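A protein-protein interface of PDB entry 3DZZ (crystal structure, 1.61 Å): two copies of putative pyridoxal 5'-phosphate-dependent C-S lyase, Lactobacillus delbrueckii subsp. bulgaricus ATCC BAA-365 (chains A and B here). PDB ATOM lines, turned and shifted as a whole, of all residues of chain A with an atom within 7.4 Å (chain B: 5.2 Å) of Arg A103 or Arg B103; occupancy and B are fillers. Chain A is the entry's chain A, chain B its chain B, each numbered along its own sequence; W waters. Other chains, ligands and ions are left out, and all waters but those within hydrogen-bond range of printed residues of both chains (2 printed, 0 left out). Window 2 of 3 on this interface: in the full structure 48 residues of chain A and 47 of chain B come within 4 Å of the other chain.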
ATOM      1  N   PRO A  96       3.990  11.479  28.408  1.00  0.00           N
ATOM      2  CA  PRO A  96       4.671  10.829  27.291  1.00  0.00           C
ATOM      3  C   PRO A  96       5.669   9.729  27.688  1.00  0.00           C
ATOM      4  O   PRO A  96       5.785   8.711  26.980  1.00  0.00           O
ATOM      5  CB  PRO A  96       5.397  11.988  26.609  1.00  0.00           C
ATOM      6  CG  PRO A  96       4.569  13.168  26.881  1.00  0.00           C
ATOM      7  CD  PRO A  96       4.085  12.948  28.326  1.00  0.00           C
ATOM      8  N   ALA A  97       6.407   9.920  28.788  1.00  0.00           N
ATOM      9  CA  ALA A  97       7.323   8.883  29.268  1.00  0.00           C
ATOM     10  C   ALA A  97       6.533   7.632  29.645  1.00  0.00           C
ATOM     11  O   ALA A  97       6.937   6.521  29.308  1.00  0.00           O
ATOM     12  CB  ALA A  97       8.107   9.403  30.443  1.00  0.00           C
ATOM     13  N   ILE A  98       5.396   7.802  30.309  1.00  0.00           N
ATOM     14  CA  ILE A  98       4.519   6.675  30.664  1.00  0.00           C
ATOM     15  C   ILE A  98       4.077   5.940  29.371  1.00  0.00           C
ATOM     16  O   ILE A  98       4.144   4.709  29.287  1.00  0.00           O
ATOM     17  CB  ILE A  98       3.306   7.072  31.487  1.00  0.00           C
ATOM     18  CG1 ILE A  98       3.727   7.667  32.830  1.00  0.00           C
ATOM     19  CG2 ILE A  98       2.401   5.834  31.754  1.00  0.00           C
ATOM     20  CD1 ILE A  98       2.583   8.307  33.647  1.00  0.00           C
ATOM     21  N   SER A  99       3.612   6.713  28.384  1.00  0.00           N
ATOM     22  CA  SER A  99       3.167   6.137  27.120  1.00  0.00           C
ATOM     23  C   SER A  99       4.274   5.253  26.499  1.00  0.00           C
ATOM     24  O   SER A  99       4.087   4.143  26.062  1.00  0.00           O
ATOM     25  CB  SER A  99       2.665   7.281  26.236  1.00  0.00           C
ATOM     26  OG  SER A  99       2.149   6.748  25.053  1.00  0.00           O
ATOM     27  N   ALA A 100       5.505   5.800  26.444  1.00  0.00           N
ATOM     28  CA  ALA A 100       6.649   5.106  25.889  1.00  0.00           C
ATOM     29  C   ALA A 100       6.952   3.822  26.667  1.00  0.00           C
ATOM     30  O   ALA A 100       7.215   2.770  26.073  1.00  0.00           O
ATOM     31  CB  ALA A 100       7.870   6.027  25.852  1.00  0.00           C
ATOM     32  N   MET A 101       6.861   3.897  27.980  1.00  0.00           N
ATOM     33  CA  MET A 101       7.150   2.729  28.800  1.00  0.00           C
ATOM     34  C   MET A 101       6.057   1.673  28.749  1.00  0.00           C
ATOM     35  O   MET A 101       6.353   0.503  28.809  1.00  0.00           O
ATOM     36  CB  MET A 101       7.431   3.170  30.222  1.00  0.00           C
ATOM     37  CG  MET A 101       8.737   3.982  30.251  1.00  0.00           C
ATOM     38  SD  MET A 101       9.351   4.319  32.033  1.00  0.00           S
ATOM     39  CE  MET A 101       7.921   5.399  32.615  1.00  0.00           C
ATOM     40  N   VAL A 102       4.811   2.088  28.555  1.00  0.00           N
ATOM     41  CA  VAL A 102       3.716   1.134  28.260  1.00  0.00           C
ATOM     42  C   VAL A 102       4.069   0.282  27.011  1.00  0.00           C
ATOM     43  O   VAL A 102       3.952  -0.949  26.998  1.00  0.00           O
ATOM     44  CB  VAL A 102       2.364   1.850  28.113  1.00  0.00           C
ATOM     45  CG1 VAL A 102       1.278   0.901  27.457  1.00  0.00           C
ATOM     46  CG2 VAL A 102       1.865   2.399  29.498  1.00  0.00           C
ATOM     47  N   ARG A 103       4.518   0.936  25.961  1.00  0.00           N
ATOM     48  CA  ARG A 103       4.829   0.238  24.736  1.00  0.00           C
ATOM     49  C   ARG A 103       6.080  -0.644  24.891  1.00  0.00           C
ATOM     50  O   ARG A 103       6.179  -1.705  24.290  1.00  0.00           O
ATOM     51  CB  ARG A 103       5.009   1.214  23.576  1.00  0.00           C
ATOM     52  CG  ARG A 103       3.774   1.972  23.121  1.00  0.00           C
ATOM     53  CD  ARG A 103       3.992   2.677  21.804  1.00  0.00           C
ATOM     54  NE  ARG A 103       4.945   3.747  22.024  1.00  0.00           N
ATOM     55  CZ  ARG A 103       4.625   4.930  22.541  1.00  0.00           C
ATOM     56  NH1 ARG A 103       3.364   5.267  22.830  1.00  0.00           N
ATOM     57  NH2 ARG A 103       5.557   5.812  22.714  1.00  0.00           N
ATOM     58  N   GLN A 104       7.053  -0.195  25.668  1.00  0.00           N
ATOM     59  CA  GLN A 104       8.314  -0.923  25.815  1.00  0.00           C
ATOM     60  C   GLN A 104       8.216  -2.121  26.745  1.00  0.00           C
ATOM     61  O   GLN A 104       8.907  -3.134  26.511  1.00  0.00           O
ATOM     62  CB  GLN A 104       9.432   0.002  26.326  1.00  0.00           C
ATOM     63  CG  GLN A 104      10.805  -0.506  26.069  1.00  0.00           C
ATOM     64  CD  GLN A 104      11.071  -0.553  24.563  1.00  0.00           C
ATOM     65  OE1 GLN A 104      10.628   0.344  23.810  1.00  0.00           O
ATOM     66  NE2 GLN A 104      11.653  -1.648  24.092  1.00  0.00           N
ATOM     67  N   PHE A 105       7.450  -1.991  27.818  1.00  0.00           N
ATOM     68  CA  PHE A 105       7.491  -2.933  28.926  1.00  0.00           C
ATOM     69  C   PHE A 105       6.255  -3.803  29.100  1.00  0.00           C
ATOM     70  O   PHE A 105       6.216  -4.612  30.011  1.00  0.00           O
ATOM     71  CB  PHE A 105       7.781  -2.241  30.218  1.00  0.00           C
ATOM     72  CG  PHE A 105       9.104  -1.492  30.223  1.00  0.00           C
ATOM     73  CD1 PHE A 105      10.242  -2.092  29.714  1.00  0.00           C
ATOM     74  CD2 PHE A 105       9.189  -0.243  30.741  1.00  0.00           C
ATOM     75  CE1 PHE A 105      11.449  -1.407  29.709  1.00  0.00           C
ATOM     76  CE2 PHE A 105      10.396   0.427  30.749  1.00  0.00           C
ATOM     77  CZ  PHE A 105      11.495  -0.146  30.230  1.00  0.00           C
ATOM     78  N   THR A 106       5.279  -3.648  28.209  1.00  0.00           N
ATOM     79  CA  THR A 106       4.110  -4.522  28.177  1.00  0.00           C
ATOM     80  C   THR A 106       3.799  -4.850  26.747  1.00  0.00           C
ATOM     81  O   THR A 106       4.405  -4.279  25.815  1.00  0.00           O
ATOM     82  CB  THR A 106       2.860  -3.851  28.808  1.00  0.00           C
ATOM     83  OG1 THR A 106       2.364  -2.784  27.987  1.00  0.00           O
ATOM     84  CG2 THR A 106       3.140  -3.277  30.214  1.00  0.00           C
ATOM     85  N   SER A 107       2.871  -5.790  26.540  1.00  0.00           N
ATOM     86  CA  SER A 107       2.438  -6.170  25.202  1.00  0.00           C
ATOM     87  C   SER A 107       0.928  -5.766  25.012  1.00  0.00           C
ATOM     88  O   SER A 107       0.215  -5.619  26.016  1.00  0.00           O
ATOM     89  CB  SER A 107       2.622  -7.665  24.970  1.00  0.00           C
ATOM     90  OG  SER A 107       4.045  -7.903  24.856  1.00  0.00           O
ATOM     91  N   PRO A 108       0.517  -5.607  23.753  1.00  0.00           N
ATOM     92  CA  PRO A 108      -0.879  -5.294  23.487  1.00  0.00           C
ATOM     93  C   PRO A 108      -1.746  -6.313  24.222  1.00  0.00           C
ATOM     94  O   PRO A 108      -1.494  -7.548  24.173  1.00  0.00           O
ATOM     95  CB  PRO A 108      -0.993  -5.367  21.964  1.00  0.00           C
ATOM     96  CG  PRO A 108       0.406  -4.989  21.466  1.00  0.00           C
ATOM     97  CD  PRO A 108       1.297  -5.665  22.489  1.00  0.00           C
ATOM     98  N   ILE A 112      -2.824  -3.136  32.854  1.00  0.00           N
ATOM     99  CA  ILE A 112      -2.026  -2.192  33.630  1.00  0.00           C
ATOM    100  C   ILE A 112      -2.909  -1.679  34.765  1.00  0.00           C
ATOM    101  O   ILE A 112      -4.027  -1.227  34.532  1.00  0.00           O
ATOM    102  CB  ILE A 112      -1.459  -1.072  32.748  1.00  0.00           C
ATOM    103  CG1 ILE A 112      -0.630  -1.672  31.599  1.00  0.00           C
ATOM    104  CG2 ILE A 112      -0.734  -0.028  33.555  1.00  0.00           C
ATOM    105  CD1 ILE A 112       0.043  -0.702  30.707  1.00  0.00           C
ATOM    106  N   VAL A 125      -3.404   6.892  28.075  1.00  0.00           N
ATOM    107  CA  VAL A 125      -2.131   6.278  27.676  1.00  0.00           C
ATOM    108  C   VAL A 125      -2.162   4.782  27.736  1.00  0.00           C
ATOM    109  O   VAL A 125      -1.464   4.134  26.977  1.00  0.00           O
ATOM    110  CB  VAL A 125      -0.825   6.823  28.368  1.00  0.00           C
ATOM    111  CG1 VAL A 125      -0.726   8.327  28.168  1.00  0.00           C
ATOM    112  CG2 VAL A 125      -0.770   6.499  29.756  1.00  0.00           C
ATOM    113  N   GLY A 128      -5.216   3.935  24.862  1.00  0.00           N
ATOM    114  CA  GLY A 128      -4.784   4.444  23.549  1.00  0.00           C
ATOM    115  C   GLY A 128      -3.686   3.612  22.973  1.00  0.00           C
ATOM    116  O   GLY A 128      -3.541   3.529  21.775  1.00  0.00           O
ATOM    117  N   ASN A 129      -2.867   3.029  23.878  1.00  0.00           N
ATOM    118  CA  ASN A 129      -1.842   2.117  23.410  1.00  0.00           C
ATOM    119  C   ASN A 129      -2.299   0.659  23.305  1.00  0.00           C
ATOM    120  O   ASN A 129      -1.501  -0.221  23.047  1.00  0.00           O
ATOM    121  CB  ASN A 129      -0.601   2.185  24.329  1.00  0.00           C
ATOM    122  CG  ASN A 129       0.294   3.397  24.071  1.00  0.00           C
ATOM    123  OD1 ASN A 129       0.858   3.523  22.995  1.00  0.00           O
ATOM    124  ND2 ASN A 129       0.398   4.272  25.044  1.00  0.00           N
ATOM    125  N   ARG A 131      -3.482  -1.305  25.695  1.00  0.00           N
ATOM    126  CA  ARG A 131      -3.461  -2.068  26.928  1.00  0.00           C
ATOM    127  C   ARG A 131      -4.782  -1.869  27.643  1.00  0.00           C
ATOM    128  O   ARG A 131      -5.619  -0.993  27.286  1.00  0.00           O
ATOM    129  CB  ARG A 131      -2.214  -1.738  27.775  1.00  0.00           C
ATOM    130  CG  ARG A 131      -0.904  -2.356  27.302  1.00  0.00           C
ATOM    131  CD  ARG A 131      -0.480  -1.916  25.915  1.00  0.00           C
ATOM    132  NE  ARG A 131       0.887  -2.338  25.589  1.00  0.00           N
ATOM    133  CZ  ARG A 131       1.486  -2.195  24.422  1.00  0.00           C
ATOM    134  NH1 ARG A 131       0.823  -1.655  23.417  1.00  0.00           N
ATOM    135  NH2 ARG A 131       2.737  -2.647  24.219  1.00  0.00           N
ATOM    136  N   MET A 163       2.128  -4.094  34.812  1.00  0.00           N
ATOM    137  CA  MET A 163       2.643  -2.757  35.211  1.00  0.00           C
ATOM    138  C   MET A 163       1.589  -2.167  36.098  1.00  0.00           C
ATOM    139  O   MET A 163       0.386  -2.493  35.999  1.00  0.00           O
ATOM    140  CB  MET A 163       2.874  -1.891  33.962  1.00  0.00           C
ATOM    141  CG  MET A 163       3.169  -0.462  34.226  1.00  0.00           C
ATOM    142  SD  MET A 163       3.439   0.526  32.605  1.00  0.00           S
ATOM    143  CE  MET A 163       5.059  -0.256  32.250  1.00  0.00           C
ATOM    144  N   SER A 260      13.319   3.929  24.549  1.00  0.00           N
ATOM    145  CA  SER A 260      11.888   4.158  24.283  1.00  0.00           C
ATOM    146  C   SER A 260      11.567   5.646  24.150  1.00  0.00           C
ATOM    147  O   SER A 260      10.735   6.030  23.322  1.00  0.00           O
ATOM    148  CB  SER A 260      10.990   3.482  25.299  1.00  0.00           C
ATOM    149  OG  SER A 260      10.805   4.220  26.492  1.00  0.00           O
ATOM    150  N   PHE A 261      12.235   6.488  24.922  1.00  0.00           N
ATOM    151  CA  PHE A 261      12.042   7.921  24.863  1.00  0.00           C
ATOM    152  C   PHE A 261      12.569   8.466  23.549  1.00  0.00           C
ATOM    153  O   PHE A 261      11.914   9.266  22.877  1.00  0.00           O
ATOM    154  CB  PHE A 261      12.747   8.637  26.006  1.00  0.00           C
ATOM    155  CG  PHE A 261      12.250   8.274  27.382  1.00  0.00           C
ATOM    156  CD1 PHE A 261      11.111   7.571  27.576  1.00  0.00           C
ATOM    157  CD2 PHE A 261      12.992   8.633  28.476  1.00  0.00           C
ATOM    158  CE1 PHE A 261      10.687   7.237  28.857  1.00  0.00           C
ATOM    159  CE2 PHE A 261      12.602   8.301  29.737  1.00  0.00           C
ATOM    160  CZ  PHE A 261      11.473   7.595  29.943  1.00  0.00           C
ATOM    161  N   PHE A 262      13.725   7.969  23.137  1.00  0.00           N
ATOM    162  CA  PHE A 262      14.266   8.397  21.823  1.00  0.00           C
ATOM    163  C   PHE A 262      13.360   7.997  20.659  1.00  0.00           C
ATOM    164  O   PHE A 262      13.029   8.837  19.818  1.00  0.00           O
ATOM    165  CB  PHE A 262      15.721   7.973  21.725  1.00  0.00           C
ATOM    166  CG  PHE A 262      16.581   8.705  22.739  1.00  0.00           C
ATOM    167  CD1 PHE A 262      16.258   8.610  24.086  1.00  0.00           C
ATOM    168  CD2 PHE A 262      17.617   9.536  22.368  1.00  0.00           C
ATOM    169  CE1 PHE A 262      16.968   9.263  25.019  1.00  0.00           C
ATOM    170  CE2 PHE A 262      18.366  10.200  23.331  1.00  0.00           C
ATOM    171  CZ  PHE A 262      18.054  10.055  24.640  1.00  0.00           C
ATOM    172  N   LEU A 263      12.826   6.794  20.692  1.00  0.00           N
ATOM    173  CA  LEU A 263      11.849   6.316  19.684  1.00  0.00           C
ATOM    174  C   LEU A 263      10.614   7.172  19.608  1.00  0.00           C
ATOM    175  O   LEU A 263      10.011   7.325  18.530  1.00  0.00           O
ATOM    176  CB  LEU A 263      11.353   4.902  19.964  1.00  0.00           C
ATOM    177  CG  LEU A 263      12.199   3.702  19.576  1.00  0.00           C
ATOM    178  CD1 LEU A 263      11.306   2.474  19.783  1.00  0.00           C
ATOM    179  CD2 LEU A 263      12.720   3.828  18.150  1.00  0.00           C
ATOM    180  N   ALA A 264      10.150   7.664  20.749  1.00  0.00           N
ATOM    181  CA  ALA A 264       8.904   8.405  20.791  1.00  0.00           C
ATOM    182  C   ALA A 264       9.153   9.857  20.316  1.00  0.00           C
ATOM    183  O   ALA A 264       8.225  10.590  20.011  1.00  0.00           O
ATOM    184  CB  ALA A 264       8.229   8.355  22.158  1.00  0.00           C
ATOM    185  N   GLY A 265      10.405  10.256  20.337  1.00  0.00           N
ATOM    186  CA  GLY A 265      10.794  11.620  20.024  1.00  0.00           C
ATOM    187  C   GLY A 265      10.654  12.544  21.213  1.00  0.00           C
ATOM    188  O   GLY A 265      10.386  13.742  21.062  1.00  0.00           O
ATOM    189  N   ILE A 266      10.859  11.989  22.426  1.00  0.00           N
ATOM    190  CA  ILE A 266      10.704  12.743  23.679  1.00  0.00           C
ATOM    191  C   ILE A 266      11.981  12.754  24.514  1.00  0.00           C
ATOM    192  O   ILE A 266      11.934  13.151  25.677  1.00  0.00           O
ATOM    193  CB  ILE A 266       9.535  12.238  24.552  1.00  0.00           C
ATOM    194  CG1 ILE A 266       9.754  10.811  25.038  1.00  0.00           C
ATOM    195  CG2 ILE A 266       8.235  12.370  23.760  1.00  0.00           C
ATOM    196  CD1 ILE A 266       8.615  10.293  25.998  1.00  0.00           C
ATOM    197  N   ILE B  98       7.547  11.219  12.045  1.00  0.00           N
ATOM    198  CA  ILE B  98       7.766  10.017  11.214  1.00  0.00           C
ATOM    199  C   ILE B  98       7.653   8.768  12.084  1.00  0.00           C
ATOM    200  O   ILE B  98       6.973   7.797  11.778  1.00  0.00           O
ATOM    201  CB  ILE B  98       9.105  10.048  10.489  1.00  0.00           C
ATOM    202  CG1 ILE B  98       9.167  11.225   9.507  1.00  0.00           C
ATOM    203  CG2 ILE B  98       9.363   8.661   9.784  1.00  0.00           C
ATOM    204  CD1 ILE B  98      10.631  11.507   8.930  1.00  0.00           C
ATOM    205  N   SER B  99       8.292   8.813  13.254  1.00  0.00           N
ATOM    206  CA  SER B  99       8.259   7.701  14.195  1.00  0.00           C
ATOM    207  C   SER B  99       6.826   7.307  14.609  1.00  0.00           C
ATOM    208  O   SER B  99       6.444   6.124  14.650  1.00  0.00           O
ATOM    209  CB  SER B  99       9.171   7.980  15.413  1.00  0.00           C
ATOM    210  OG  SER B  99       9.412   6.850  16.243  1.00  0.00           O
ATOM    211  N   ALA B 100       6.037   8.323  15.004  1.00  0.00           N
ATOM    212  CA  ALA B 100       4.613   8.085  15.339  1.00  0.00           C
ATOM    213  C   ALA B 100       3.861   7.401  14.196  1.00  0.00           C
ATOM    214  O   ALA B 100       3.033   6.512  14.400  1.00  0.00           O
ATOM    215  CB  ALA B 100       3.896   9.390  15.798  1.00  0.00           C
ATOM    216  N   MET B 101       4.099   7.880  12.993  1.00  0.00           N
ATOM    217  CA  MET B 101       3.381   7.374  11.816  1.00  0.00           C
ATOM    218  C   MET B 101       3.863   5.972  11.432  1.00  0.00           C
ATOM    219  O   MET B 101       3.082   5.160  10.973  1.00  0.00           O
ATOM    220  CB  MET B 101       3.444   8.358  10.670  1.00  0.00           C
ATOM    221  CG  MET B 101       2.640   9.649  10.987  1.00  0.00           C
ATOM    222  SD  MET B 101       2.545  10.885   9.514  1.00  0.00           S
ATOM    223  CE  MET B 101       4.356  11.229   9.273  1.00  0.00           C
ATOM    224  N   VAL B 102       5.144   5.684  11.612  1.00  0.00           N
ATOM    225  CA  VAL B 102       5.631   4.307  11.457  1.00  0.00           C
ATOM    226  C   VAL B 102       4.778   3.407  12.365  1.00  0.00           C
ATOM    227  O   VAL B 102       4.264   2.355  11.982  1.00  0.00           O
ATOM    228  CB  VAL B 102       7.086   4.204  11.838  1.00  0.00           C
ATOM    229  CG1 VAL B 102       7.509   2.730  12.023  1.00  0.00           C
ATOM    230  CG2 VAL B 102       7.928   4.847  10.769  1.00  0.00           C
ATOM    231  N   ARG B 103       4.634   3.765  13.640  1.00  0.00           N
ATOM    232  CA  ARG B 103       3.858   2.921  14.527  1.00  0.00           C
ATOM    233  C   ARG B 103       2.368   2.852  14.165  1.00  0.00           C
ATOM    234  O   ARG B 103       1.718   1.809  14.348  1.00  0.00           O
ATOM    235  CB  ARG B 103       4.027   3.355  16.004  1.00  0.00           C
ATOM    236  CG  ARG B 103       5.447   3.103  16.583  1.00  0.00           C
ATOM    237  CD  ARG B 103       5.534   3.361  18.093  1.00  0.00           C
ATOM    238  NE  ARG B 103       5.084   4.714  18.438  1.00  0.00           N
ATOM    239  CZ  ARG B 103       5.916   5.754  18.297  1.00  0.00           C
ATOM    240  NH1 ARG B 103       7.190   5.579  17.941  1.00  0.00           N
ATOM    241  NH2 ARG B 103       5.510   6.974  18.571  1.00  0.00           N
ATOM    242  N   GLN B 104       1.783   3.929  13.673  1.00  0.00           N
ATOM    243  CA  GLN B 104       0.343   3.930  13.431  1.00  0.00           C
ATOM    244  C   GLN B 104      -0.030   3.267  12.107  1.00  0.00           C
ATOM    245  O   GLN B 104      -1.072   2.591  12.028  1.00  0.00           O
ATOM    246  CB  GLN B 104      -0.222   5.375  13.479  1.00  0.00           C
ATOM    247  CG  GLN B 104      -1.701   5.445  13.683  1.00  0.00           C
ATOM    248  CD  GLN B 104      -1.980   5.002  15.050  1.00  0.00           C
ATOM    249  OE1 GLN B 104      -1.280   5.414  16.000  1.00  0.00           O
ATOM    250  NE2 GLN B 104      -2.931   4.120  15.206  1.00  0.00           N
ATOM    251  N   PHE B 105       0.826   3.439  11.076  1.00  0.00           N
ATOM    252  CA  PHE B 105       0.447   3.123   9.717  1.00  0.00           C
ATOM    253  C   PHE B 105       1.151   1.896   9.147  1.00  0.00           C
ATOM    254  O   PHE B 105       0.975   1.515   7.990  1.00  0.00           O
ATOM    255  CB  PHE B 105       0.720   4.327   8.835  1.00  0.00           C
ATOM    256  CG  PHE B 105      -0.054   5.560   9.232  1.00  0.00           C
ATOM    257  CD1 PHE B 105      -1.322   5.462   9.745  1.00  0.00           C
ATOM    258  CD2 PHE B 105       0.470   6.817   9.042  1.00  0.00           C
ATOM    259  CE1 PHE B 105      -2.042   6.618  10.103  1.00  0.00           C
ATOM    260  CE2 PHE B 105      -0.297   7.956   9.401  1.00  0.00           C
ATOM    261  CZ  PHE B 105      -1.540   7.813   9.910  1.00  0.00           C
ATOM    262  N   THR B 106       1.934   1.243   9.995  1.00  0.00           N
ATOM    263  CA  THR B 106       2.569  -0.054   9.645  1.00  0.00           C
ATOM    264  C   THR B 106       2.483  -0.958  10.853  1.00  0.00           C
ATOM    265  O   THR B 106       2.204  -0.487  11.955  1.00  0.00           O
ATOM    266  CB  THR B 106       4.046   0.099   9.188  1.00  0.00           C
ATOM    267  OG1 THR B 106       4.908   0.384  10.309  1.00  0.00           O
ATOM    268  CG2 THR B 106       4.236   1.118   8.138  1.00  0.00           C
ATOM    269  N   ASN B 129      11.860   0.993  15.871  1.00  0.00           N
ATOM    270  CA  ASN B 129      10.458   0.654  16.001  1.00  0.00           C
ATOM    271  C   ASN B 129      10.104  -0.725  15.571  1.00  0.00           C
ATOM    272  O   ASN B 129       8.947  -1.076  15.557  1.00  0.00           O
ATOM    273  CB  ASN B 129       9.557   1.650  15.218  1.00  0.00           C
ATOM    274  CG  ASN B 129       9.302   2.948  15.948  1.00  0.00           C
ATOM    275  OD1 ASN B 129       8.789   2.980  17.109  1.00  0.00           O
ATOM    276  ND2 ASN B 129       9.737   4.047  15.314  1.00  0.00           N
ATOM    277  N   ARG B 131      10.499  -2.110  12.548  1.00  0.00           N
ATOM    278  CA  ARG B 131      10.225  -2.241  11.129  1.00  0.00           C
ATOM    279  C   ARG B 131      11.581  -2.419  10.428  1.00  0.00           C
ATOM    280  O   ARG B 131      12.673  -2.335  11.068  1.00  0.00           O
ATOM    281  CB  ARG B 131       9.390  -1.088  10.606  1.00  0.00           C
ATOM    282  CG  ARG B 131       7.916  -1.079  10.896  1.00  0.00           C
ATOM    283  CD  ARG B 131       7.625  -0.983  12.371  1.00  0.00           C
ATOM    284  NE  ARG B 131       6.167  -0.771  12.591  1.00  0.00           N
ATOM    285  CZ  ARG B 131       5.565  -0.822  13.776  1.00  0.00           C
ATOM    286  NH1 ARG B 131       6.243  -1.048  14.888  1.00  0.00           N
ATOM    287  NH2 ARG B 131       4.255  -0.625  13.894  1.00  0.00           N
ATOM    288  N   LEU B 263      -0.676  10.602  21.282  1.00  0.00           N
ATOM    289  CA  LEU B 263      -0.339   9.347  21.989  1.00  0.00           C
ATOM    290  C   LEU B 263       1.147   9.293  22.320  1.00  0.00           C
ATOM    291  O   LEU B 263       1.524   8.857  23.434  1.00  0.00           O
ATOM    292  CB  LEU B 263      -0.729   8.145  21.140  1.00  0.00           C
ATOM    293  CG  LEU B 263      -0.529   6.735  21.757  1.00  0.00           C
ATOM    294  CD1 LEU B 263      -1.391   6.598  22.979  1.00  0.00           C
ATOM    295  CD2 LEU B 263      -0.847   5.645  20.726  1.00  0.00           C
ATOM    296  N   ALA B 264       1.995   9.783  21.415  1.00  0.00           N
ATOM    297  CA  ALA B 264       3.465   9.753  21.605  1.00  0.00           C
ATOM    298  C   ALA B 264       3.932  10.915  22.506  1.00  0.00           C
ATOM    299  O   ALA B 264       5.008  10.863  23.069  1.00  0.00           O
ATOM    300  CB  ALA B 264       4.132   9.845  20.302  1.00  0.00           C
HETATM  301  O   HOH W   1       5.505   8.372  24.222  1.00  0.00           O
HETATM  302  O   HOH W   2       6.871   9.398  17.942  1.00  0.00           O
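The side-chain hydroxyl (OG) of Ser A99 is in hydrogen-bond range of the backbone carbonyl oxygen (O) of Leu B263, at 2.7 Å.
O of Leu A263 is in hydrogen-bond range of OG of Ser B99.
O of Leu A263 lies within hydrogen-bond range of NH1 of Arg B103, at 3.4 Å.
The side-chain hydroxyl of Ser B99 lies within hydrogen-bond range of the side-chain amide nitrogen of Asn B129, 3.0 Å away.
The guanidinium group of Arg B103 is in hydrogen-bond range of the side-chain amide oxygen of Asn B129.
O of Asn A129 sits at hydrogen-bond distance from NH1 of Arg A131 (2.8 Å).
The side-chain amide oxygen (OD1) of Asn A129 lies within hydrogen-bond range of the guanidinium group (NH1) of Arg A103.
The backbone carbonyl oxygen (O) of Phe A261 lies within hydrogen-bond range of the backbone NH (N) of Ile A266, at 3.0 Å.
The side-chain hydroxyl (OG) of Ser B99 sits at hydrogen-bond distance from the guanidinium group (NH1) of Arg B103, at 3.1 Å.
Among the printed residues, pairs that only touch across the chains: Asn A129 with Leu B263 (3.5 Å), Gly A128 with Leu B263 (3.6 Å), Ile A266 with Ala B264 (3.6 Å), Leu A263 with Asn B129 (3.7 Å), Arg A103 with Arg B103 (3.7 Å) and Pro A96 with Ala B264 (3.7 Å).
Of the printed residues of chain B, Ser A99 touches Leu B263.
Of the printed residues of chain B, Arg A103 touches Arg B103 (3.7 Å).
Ile A112 touches none of the printed residues of chain B.
Val A125 touches none of the printed residues of chain B.
Of the printed residues of chain B, Gly A128 touches Leu B263.
Of the printed residues of chain B, Asn A129 touches Leu B263.
Of the printed residues of chain B, Leu A263 touches Ser B99 (2.4 Å), Arg B103 (3.4 Å) and Asn B129 (3.7 Å).
Arg B103 touches two residues of chain A.
The nearest residue of chain A that does not touch Arg B103 is Ala A264 (4.3 Å).
Hydrophobic or aromatic side chains of chain A within 4 Å of the printed part of chain B: Pro A96, Leu A263 and Ile A266.
Of the 13 printed residues of chain B, 5 touch a printed residue of chain A.
Hydrophobic or aromatic side chains of chain B that line the printed part of chain A: Leu B263.
Among the printed residues, 9 pairs touch across the chains.
Among the printed residues, no Asp or Glu carboxylate lies within 4 Å of a Lys or Arg side-chain nitrogen of the other chain.
Ser A99 touches Leu B263, and with the chains exchanged Leu A263 touches Ser B99.
Arg B103 touches its own counterpart, Arg A103.
Asn A129 touches Leu B263, and with the chains exchanged Leu A263 touches Asn B129.
Leu A263 touches Arg B103, but with the chains exchanged Arg A103 does not touch Leu B263 (4.1 Å).
Water W2 lies within hydrogen-bond range of O of Ala A264 (2.7 Å), NH2 of Arg B103 (2.9 Å) and N of Ala B100 (3.2 Å).
Water W1 lies within hydrogen-bond range of O of Ala B264, O of Pro A96, NH2 of Arg A103 and N of Ala A100.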
